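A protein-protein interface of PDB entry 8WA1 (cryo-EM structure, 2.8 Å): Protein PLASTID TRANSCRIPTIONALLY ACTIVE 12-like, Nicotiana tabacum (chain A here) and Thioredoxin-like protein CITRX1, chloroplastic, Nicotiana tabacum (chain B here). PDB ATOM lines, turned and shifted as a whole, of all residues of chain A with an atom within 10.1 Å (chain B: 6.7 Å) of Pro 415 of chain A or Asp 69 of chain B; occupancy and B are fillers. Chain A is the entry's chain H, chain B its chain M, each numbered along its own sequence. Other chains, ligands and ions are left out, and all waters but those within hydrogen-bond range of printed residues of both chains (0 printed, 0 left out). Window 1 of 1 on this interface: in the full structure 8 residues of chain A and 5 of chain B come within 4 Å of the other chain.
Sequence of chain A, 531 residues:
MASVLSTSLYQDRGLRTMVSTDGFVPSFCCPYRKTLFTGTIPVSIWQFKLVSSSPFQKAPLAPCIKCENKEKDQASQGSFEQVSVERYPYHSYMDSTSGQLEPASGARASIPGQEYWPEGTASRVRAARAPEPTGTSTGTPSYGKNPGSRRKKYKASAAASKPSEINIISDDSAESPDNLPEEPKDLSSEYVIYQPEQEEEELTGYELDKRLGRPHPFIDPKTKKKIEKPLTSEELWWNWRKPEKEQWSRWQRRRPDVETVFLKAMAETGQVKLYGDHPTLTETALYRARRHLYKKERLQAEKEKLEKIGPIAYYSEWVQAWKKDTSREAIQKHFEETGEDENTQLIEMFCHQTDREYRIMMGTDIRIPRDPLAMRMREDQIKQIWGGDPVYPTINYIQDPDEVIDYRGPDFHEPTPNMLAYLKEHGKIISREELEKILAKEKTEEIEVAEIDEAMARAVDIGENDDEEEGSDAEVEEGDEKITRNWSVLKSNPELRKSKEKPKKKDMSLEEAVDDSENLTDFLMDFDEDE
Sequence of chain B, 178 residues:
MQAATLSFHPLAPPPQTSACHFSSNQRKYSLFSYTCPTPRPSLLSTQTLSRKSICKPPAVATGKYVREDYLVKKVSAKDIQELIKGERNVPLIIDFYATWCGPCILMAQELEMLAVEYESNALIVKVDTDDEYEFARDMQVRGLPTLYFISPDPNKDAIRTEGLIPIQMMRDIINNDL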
ATOM      1  N   ASP A 406     -27.062  27.724  13.247  1.00  0.00           N
ATOM      2  CA  ASP A 406     -26.493  26.404  13.017  1.00  0.00           C
ATOM      3  C   ASP A 406     -27.025  25.442  14.073  1.00  0.00           C
ATOM      4  O   ASP A 406     -26.722  25.588  15.262  1.00  0.00           O
ATOM      5  CB  ASP A 406     -24.969  26.463  13.056  1.00  0.00           C
ATOM      6  CG  ASP A 406     -24.322  25.150  12.659  1.00  0.00           C
ATOM      7  OD1 ASP A 406     -25.039  24.242  12.191  1.00  0.00           O
ATOM      8  OD2 ASP A 406     -23.089  25.026  12.818  1.00  0.00           O
ATOM      9  N   TYR A 407     -27.810  24.460  13.640  1.00  0.00           N
ATOM     10  CA  TYR A 407     -28.400  23.487  14.548  1.00  0.00           C
ATOM     11  C   TYR A 407     -27.428  22.389  14.958  1.00  0.00           C
ATOM     12  O   TYR A 407     -27.827  21.462  15.669  1.00  0.00           O
ATOM     13  CB  TYR A 407     -29.649  22.866  13.914  1.00  0.00           C
ATOM     14  CG  TYR A 407     -30.754  23.861  13.647  1.00  0.00           C
ATOM     15  CD1 TYR A 407     -31.466  24.433  14.692  1.00  0.00           C
ATOM     16  CD2 TYR A 407     -31.091  24.225  12.350  1.00  0.00           C
ATOM     17  CE1 TYR A 407     -32.479  25.342  14.455  1.00  0.00           C
ATOM     18  CE2 TYR A 407     -32.104  25.134  12.103  1.00  0.00           C
ATOM     19  CZ  TYR A 407     -32.794  25.688  13.158  1.00  0.00           C
ATOM     20  OH  TYR A 407     -33.802  26.592  12.921  1.00  0.00           O
ATOM     21  N   ARG A 408     -26.170  22.468  14.526  1.00  0.00           N
ATOM     22  CA  ARG A 408     -25.131  21.536  14.940  1.00  0.00           C
ATOM     23  C   ARG A 408     -24.246  22.111  16.040  1.00  0.00           C
ATOM     24  O   ARG A 408     -23.123  21.635  16.237  1.00  0.00           O
ATOM     25  CB  ARG A 408     -24.280  21.124  13.736  1.00  0.00           C
ATOM     26  CG  ARG A 408     -25.030  20.303  12.701  1.00  0.00           C
ATOM     27  CD  ARG A 408     -25.297  18.894  13.201  1.00  0.00           C
ATOM     28  NE  ARG A 408     -24.059  18.142  13.389  1.00  0.00           N
ATOM     29  CZ  ARG A 408     -24.005  16.879  13.795  1.00  0.00           C
ATOM     30  NH1 ARG A 408     -22.833  16.275  13.936  1.00  0.00           N
ATOM     31  NH2 ARG A 408     -25.122  16.217  14.062  1.00  0.00           N
ATOM     32  N   GLY A 409     -24.727  23.123  16.755  1.00  0.00           N
ATOM     33  CA  GLY A 409     -23.962  23.739  17.815  1.00  0.00           C
ATOM     34  C   GLY A 409     -24.010  22.933  19.093  1.00  0.00           C
ATOM     35  O   GLY A 409     -24.648  21.874  19.190  1.00  0.00           O
ATOM     36  N   PHE A 412     -27.695  22.645  20.940  1.00  0.00           N
ATOM     37  CA  PHE A 412     -28.787  21.930  20.300  1.00  0.00           C
ATOM     38  C   PHE A 412     -28.599  20.428  20.458  1.00  0.00           C
ATOM     39  O   PHE A 412     -27.475  19.932  20.583  1.00  0.00           O
ATOM     40  CB  PHE A 412     -28.888  22.290  18.814  1.00  0.00           C
ATOM     41  CG  PHE A 412     -29.306  23.710  18.565  1.00  0.00           C
ATOM     42  CD1 PHE A 412     -30.646  24.063  18.580  1.00  0.00           C
ATOM     43  CD2 PHE A 412     -28.363  24.692  18.317  1.00  0.00           C
ATOM     44  CE1 PHE A 412     -31.035  25.368  18.354  1.00  0.00           C
ATOM     45  CE2 PHE A 412     -28.746  25.998  18.089  1.00  0.00           C
ATOM     46  CZ  PHE A 412     -30.084  26.337  18.107  1.00  0.00           C
ATOM     47  N   HIS A 413     -29.717  19.707  20.454  1.00  0.00           N
ATOM     48  CA  HIS A 413     -29.690  18.264  20.618  1.00  0.00           C
ATOM     49  C   HIS A 413     -29.270  17.583  19.316  1.00  0.00           C
ATOM     50  O   HIS A 413     -29.022  18.225  18.292  1.00  0.00           O
ATOM     51  CB  HIS A 413     -31.057  17.752  21.069  1.00  0.00           C
ATOM     52  CG  HIS A 413     -32.157  18.026  20.092  1.00  0.00           C
ATOM     53  ND1 HIS A 413     -32.333  17.287  18.942  1.00  0.00           N
ATOM     54  CD2 HIS A 413     -33.136  18.961  20.091  1.00  0.00           C
ATOM     55  CE1 HIS A 413     -33.374  17.753  18.276  1.00  0.00           C
ATOM     56  NE2 HIS A 413     -33.880  18.770  18.951  1.00  0.00           N
ATOM     57  N   GLU A 414     -29.195  16.255  19.369  1.00  0.00           N
ATOM     58  CA  GLU A 414     -28.843  15.482  18.192  1.00  0.00           C
ATOM     59  C   GLU A 414     -29.942  15.599  17.136  1.00  0.00           C
ATOM     60  O   GLU A 414     -31.111  15.815  17.469  1.00  0.00           O
ATOM     61  CB  GLU A 414     -28.625  14.016  18.564  1.00  0.00           C
ATOM     62  CG  GLU A 414     -27.478  13.792  19.535  1.00  0.00           C
ATOM     63  CD  GLU A 414     -26.132  14.177  18.951  1.00  0.00           C
ATOM     64  OE1 GLU A 414     -25.963  14.073  17.717  1.00  0.00           O
ATOM     65  OE2 GLU A 414     -25.243  14.588  19.726  1.00  0.00           O
ATOM     66  N   PRO A 415     -29.592  15.474  15.856  1.00  0.00           N
ATOM     67  CA  PRO A 415     -30.609  15.571  14.802  1.00  0.00           C
ATOM     68  C   PRO A 415     -31.678  14.500  14.961  1.00  0.00           C
ATOM     69  O   PRO A 415     -31.400  13.371  15.366  1.00  0.00           O
ATOM     70  CB  PRO A 415     -29.803  15.375  13.512  1.00  0.00           C
ATOM     71  CG  PRO A 415     -28.417  15.778  13.873  1.00  0.00           C
ATOM     72  CD  PRO A 415     -28.233  15.359  15.300  1.00  0.00           C
ATOM     73  N   THR A 416     -32.910  14.870  14.636  1.00  0.00           N
ATOM     74  CA  THR A 416     -34.023  13.944  14.787  1.00  0.00           C
ATOM     75  C   THR A 416     -34.001  12.906  13.666  1.00  0.00           C
ATOM     76  O   THR A 416     -34.022  13.264  12.486  1.00  0.00           O
ATOM     77  CB  THR A 416     -35.353  14.694  14.769  1.00  0.00           C
ATOM     78  OG1 THR A 416     -35.388  15.633  15.851  1.00  0.00           O
ATOM     79  CG2 THR A 416     -36.513  13.721  14.915  1.00  0.00           C
ATOM     80  N   PRO A 417     -33.957  11.620  14.006  1.00  0.00           N
ATOM     81  CA  PRO A 417     -33.964  10.582  12.969  1.00  0.00           C
ATOM     82  C   PRO A 417     -35.360  10.330  12.425  1.00  0.00           C
ATOM     83  O   PRO A 417     -36.333  10.307  13.184  1.00  0.00           O
ATOM     84  CB  PRO A 417     -33.418   9.345  13.699  1.00  0.00           C
ATOM     85  CG  PRO A 417     -32.894   9.848  15.023  1.00  0.00           C
ATOM     86  CD  PRO A 417     -33.705  11.057  15.340  1.00  0.00           C
ATOM     87  N   ASN A 418     -35.466  10.162  11.109  1.00  0.00           N
ATOM     88  CA  ASN A 418     -36.741   9.815  10.497  1.00  0.00           C
ATOM     89  C   ASN A 418     -37.249   8.495  11.063  1.00  0.00           C
ATOM     90  O   ASN A 418     -36.489   7.532  11.198  1.00  0.00           O
ATOM     91  CB  ASN A 418     -36.584   9.727   8.980  1.00  0.00           C
ATOM     92  CG  ASN A 418     -37.897   9.474   8.270  1.00  0.00           C
ATOM     93  OD1 ASN A 418     -38.684  10.394   8.050  1.00  0.00           O
ATOM     94  ND2 ASN A 418     -38.136   8.222   7.898  1.00  0.00           N
ATOM     95  N   MET A 419     -38.542   8.457  11.402  1.00  0.00           N
ATOM     96  CA  MET A 419     -39.098   7.288  12.079  1.00  0.00           C
ATOM     97  C   MET A 419     -38.962   6.031  11.231  1.00  0.00           C
ATOM     98  O   MET A 419     -38.568   4.973  11.735  1.00  0.00           O
ATOM     99  CB  MET A 419     -40.564   7.533  12.438  1.00  0.00           C
ATOM    100  CG  MET A 419     -41.230   6.359  13.138  1.00  0.00           C
ATOM    101  SD  MET A 419     -40.687   6.151  14.844  1.00  0.00           S
ATOM    102  CE  MET A 419     -41.494   7.547  15.624  1.00  0.00           C
ATOM    103  N   TYR A 422     -35.290   5.029  11.016  1.00  0.00           N
ATOM    104  CA  TYR A 422     -34.833   4.577  12.327  1.00  0.00           C
ATOM    105  C   TYR A 422     -35.354   3.181  12.639  1.00  0.00           C
ATOM    106  O   TYR A 422     -34.633   2.354  13.211  1.00  0.00           O
ATOM    107  CB  TYR A 422     -35.270   5.572  13.403  1.00  0.00           C
ATOM    108  CG  TYR A 422     -34.916   5.165  14.815  1.00  0.00           C
ATOM    109  CD1 TYR A 422     -33.640   5.371  15.320  1.00  0.00           C
ATOM    110  CD2 TYR A 422     -35.863   4.585  15.650  1.00  0.00           C
ATOM    111  CE1 TYR A 422     -33.313   5.005  16.612  1.00  0.00           C
ATOM    112  CE2 TYR A 422     -35.546   4.215  16.943  1.00  0.00           C
ATOM    113  CZ  TYR A 422     -34.270   4.427  17.419  1.00  0.00           C
ATOM    114  OH  TYR A 422     -33.952   4.060  18.706  1.00  0.00           O
ATOM    115  N   VAL B  66     -29.832   5.235   7.864  1.00  0.00           N
ATOM    116  CA  VAL B  66     -29.569   6.491   8.557  1.00  0.00           C
ATOM    117  C   VAL B  66     -28.092   6.829   8.409  1.00  0.00           C
ATOM    118  O   VAL B  66     -27.227   5.972   8.627  1.00  0.00           O
ATOM    119  CB  VAL B  66     -29.977   6.424  10.041  1.00  0.00           C
ATOM    120  CG1 VAL B  66     -31.489   6.437  10.172  1.00  0.00           C
ATOM    121  CG2 VAL B  66     -29.398   5.183  10.705  1.00  0.00           C
ATOM    122  N   ARG B  67     -27.809   8.069   8.022  1.00  0.00           N
ATOM    123  CA  ARG B  67     -26.431   8.516   7.871  1.00  0.00           C
ATOM    124  C   ARG B  67     -25.826   8.841   9.232  1.00  0.00           C
ATOM    125  O   ARG B  67     -26.526   9.266  10.156  1.00  0.00           O
ATOM    126  CB  ARG B  67     -26.372   9.739   6.956  1.00  0.00           C
ATOM    127  CG  ARG B  67     -24.967  10.183   6.585  1.00  0.00           C
ATOM    128  CD  ARG B  67     -24.213   9.078   5.863  1.00  0.00           C
ATOM    129  NE  ARG B  67     -22.850   9.475   5.526  1.00  0.00           N
ATOM    130  CZ  ARG B  67     -21.971   8.684   4.918  1.00  0.00           C
ATOM    131  NH1 ARG B  67     -22.312   7.449   4.579  1.00  0.00           N
ATOM    132  NH2 ARG B  67     -20.749   9.127   4.651  1.00  0.00           N
ATOM    133  N   GLU B  68     -24.518   8.633   9.355  1.00  0.00           N
ATOM    134  CA  GLU B  68     -23.825   8.945  10.597  1.00  0.00           C
ATOM    135  C   GLU B  68     -23.727  10.454  10.788  1.00  0.00           C
ATOM    136  O   GLU B  68     -23.481  11.202   9.838  1.00  0.00           O
ATOM    137  CB  GLU B  68     -22.427   8.324  10.604  1.00  0.00           C
ATOM    138  CG  GLU B  68     -22.409   6.808  10.747  1.00  0.00           C
ATOM    139  CD  GLU B  68     -22.807   6.089   9.472  1.00  0.00           C
ATOM    140  OE1 GLU B  68     -22.868   6.743   8.411  1.00  0.00           O
ATOM    141  OE2 GLU B  68     -23.060   4.868   9.532  1.00  0.00           O
ATOM    142  N   ASP B  69     -23.922  10.898  12.031  1.00  0.00           N
ATOM    143  CA  ASP B  69     -23.904  12.329  12.315  1.00  0.00           C
ATOM    144  C   ASP B  69     -22.489  12.891  12.268  1.00  0.00           C
ATOM    145  O   ASP B  69     -22.272  14.001  11.769  1.00  0.00           O
ATOM    146  CB  ASP B  69     -24.544  12.597  13.678  1.00  0.00           C
ATOM    147  CG  ASP B  69     -25.974  12.097  13.758  1.00  0.00           C
ATOM    148  OD1 ASP B  69     -26.478  11.563  12.747  1.00  0.00           O
ATOM    149  OD2 ASP B  69     -26.593  12.235  14.833  1.00  0.00           O
ATOM    150  N   TYR B  70     -21.515  12.144  12.781  1.00  0.00           N
ATOM    151  CA  TYR B  70     -20.132  12.593  12.863  1.00  0.00           C
ATOM    152  C   TYR B  70     -19.275  11.769  11.912  1.00  0.00           C
ATOM    153  O   TYR B  70     -19.401  10.541  11.860  1.00  0.00           O
ATOM    154  CB  TYR B  70     -19.614  12.478  14.298  1.00  0.00           C
ATOM    155  CG  TYR B  70     -20.494  13.178  15.311  1.00  0.00           C
ATOM    156  CD1 TYR B  70     -20.311  14.522  15.608  1.00  0.00           C
ATOM    157  CD2 TYR B  70     -21.514  12.497  15.965  1.00  0.00           C
ATOM    158  CE1 TYR B  70     -21.115  15.166  16.529  1.00  0.00           C
ATOM    159  CE2 TYR B  70     -22.323  13.134  16.888  1.00  0.00           C
ATOM    160  CZ  TYR B  70     -22.118  14.468  17.166  1.00  0.00           C
ATOM    161  OH  TYR B  70     -22.919  15.109  18.084  1.00  0.00           O
ATOM    162  N   LEU B  71     -18.406  12.446  11.163  1.00  0.00           N
ATOM    163  CA  LEU B  71     -17.595  11.810  10.132  1.00  0.00           C
ATOM    164  C   LEU B  71     -16.136  11.634  10.532  1.00  0.00           C
ATOM    165  O   LEU B  71     -15.365  11.053   9.762  1.00  0.00           O
ATOM    166  CB  LEU B  71     -17.674  12.609   8.827  1.00  0.00           C
ATOM    167  CG  LEU B  71     -18.861  12.359   7.891  1.00  0.00           C
ATOM    168  CD1 LEU B  71     -20.175  12.835   8.497  1.00  0.00           C
ATOM    169  CD2 LEU B  71     -18.617  13.025   6.546  1.00  0.00           C
ATOM    170  N   GLU B 112     -15.205  19.049  11.632  1.00  0.00           N
ATOM    171  CA  GLU B 112     -16.360  18.456  10.962  1.00  0.00           C
ATOM    172  C   GLU B 112     -16.643  19.154   9.638  1.00  0.00           C
ATOM    173  O   GLU B 112     -16.875  18.495   8.616  1.00  0.00           O
ATOM    174  CB  GLU B 112     -17.587  18.522  11.869  1.00  0.00           C
ATOM    175  CG  GLU B 112     -17.585  17.531  13.018  1.00  0.00           C
ATOM    176  CD  GLU B 112     -17.804  16.105  12.555  1.00  0.00           C
ATOM    177  OE1 GLU B 112     -16.814  15.352  12.453  1.00  0.00           O
ATOM    178  OE2 GLU B 112     -18.968  15.741  12.285  1.00  0.00           O
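O of Asp 69 of chain B is in hydrogen-bond range of NH1 of Arg 408 of chain A, 3.2 Å away.
The side-chain carboxylate (OE2) of Glu 414 of chain A sits at hydrogen-bond distance from the side-chain hydroxyl (OH) of Tyr 70 of chain B (2.9 Å).
OE1 of Glu 414 of chain A lies close to OD2 of Asp 69 of chain B, at 3.5 Å.
The backbone NH of Arg 408 of chain A sits close to the side-chain carboxylate of Asp 406 of chain A, 3.1 Å away.
Of the printed residues of chain B, Arg 408 of chain A touches Asp 69 (3.2 Å) and Tyr 70 (3.3 Å).
Printed residues of chain B within 4 Å of Glu 414 of chain A: Asp 69 and Tyr 70.
Asn 418 of chain A touches none of the printed residues of chain B.
Of chain A, only Arg 408, Glu 414 and Pro 415 come within 4 Å of Asp 69 of chain B.
The nearest residue of chain B that does not touch Pro 415 of chain A is Tyr 70 of chain B (6.0 Å).
The nearest residue of chain A that does not touch Asp 69 of chain B is Pro 417 of chain A (6.7 Å).
The nearest printed residue of chain B that does not touch Arg 408 of chain A is Glu 112 of chain B (4.2 Å).
Among the printed residues, merely in contact across the chains: Arg 408 of chain A with Tyr 70 of chain B (3.3 Å) and Pro 415 of chain A with Asp 69 of chain B (3.6 Å).
Of the 13 printed residues of chain A, 3 touch a printed residue of chain B.
Printed residues of chain A that touch a printed residue of chain B: Arg 408, Glu 414 and Pro 415.
Printed residues of chain B that touch a printed residue of chain A: Asp 69 and Tyr 70.
Among the printed residues, 5 pairs touch across the chains.
Among the printed residues, no Asp or Glu carboxylate lies within 4 Å of a Lys or Arg side-chain nitrogen of the other chain.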
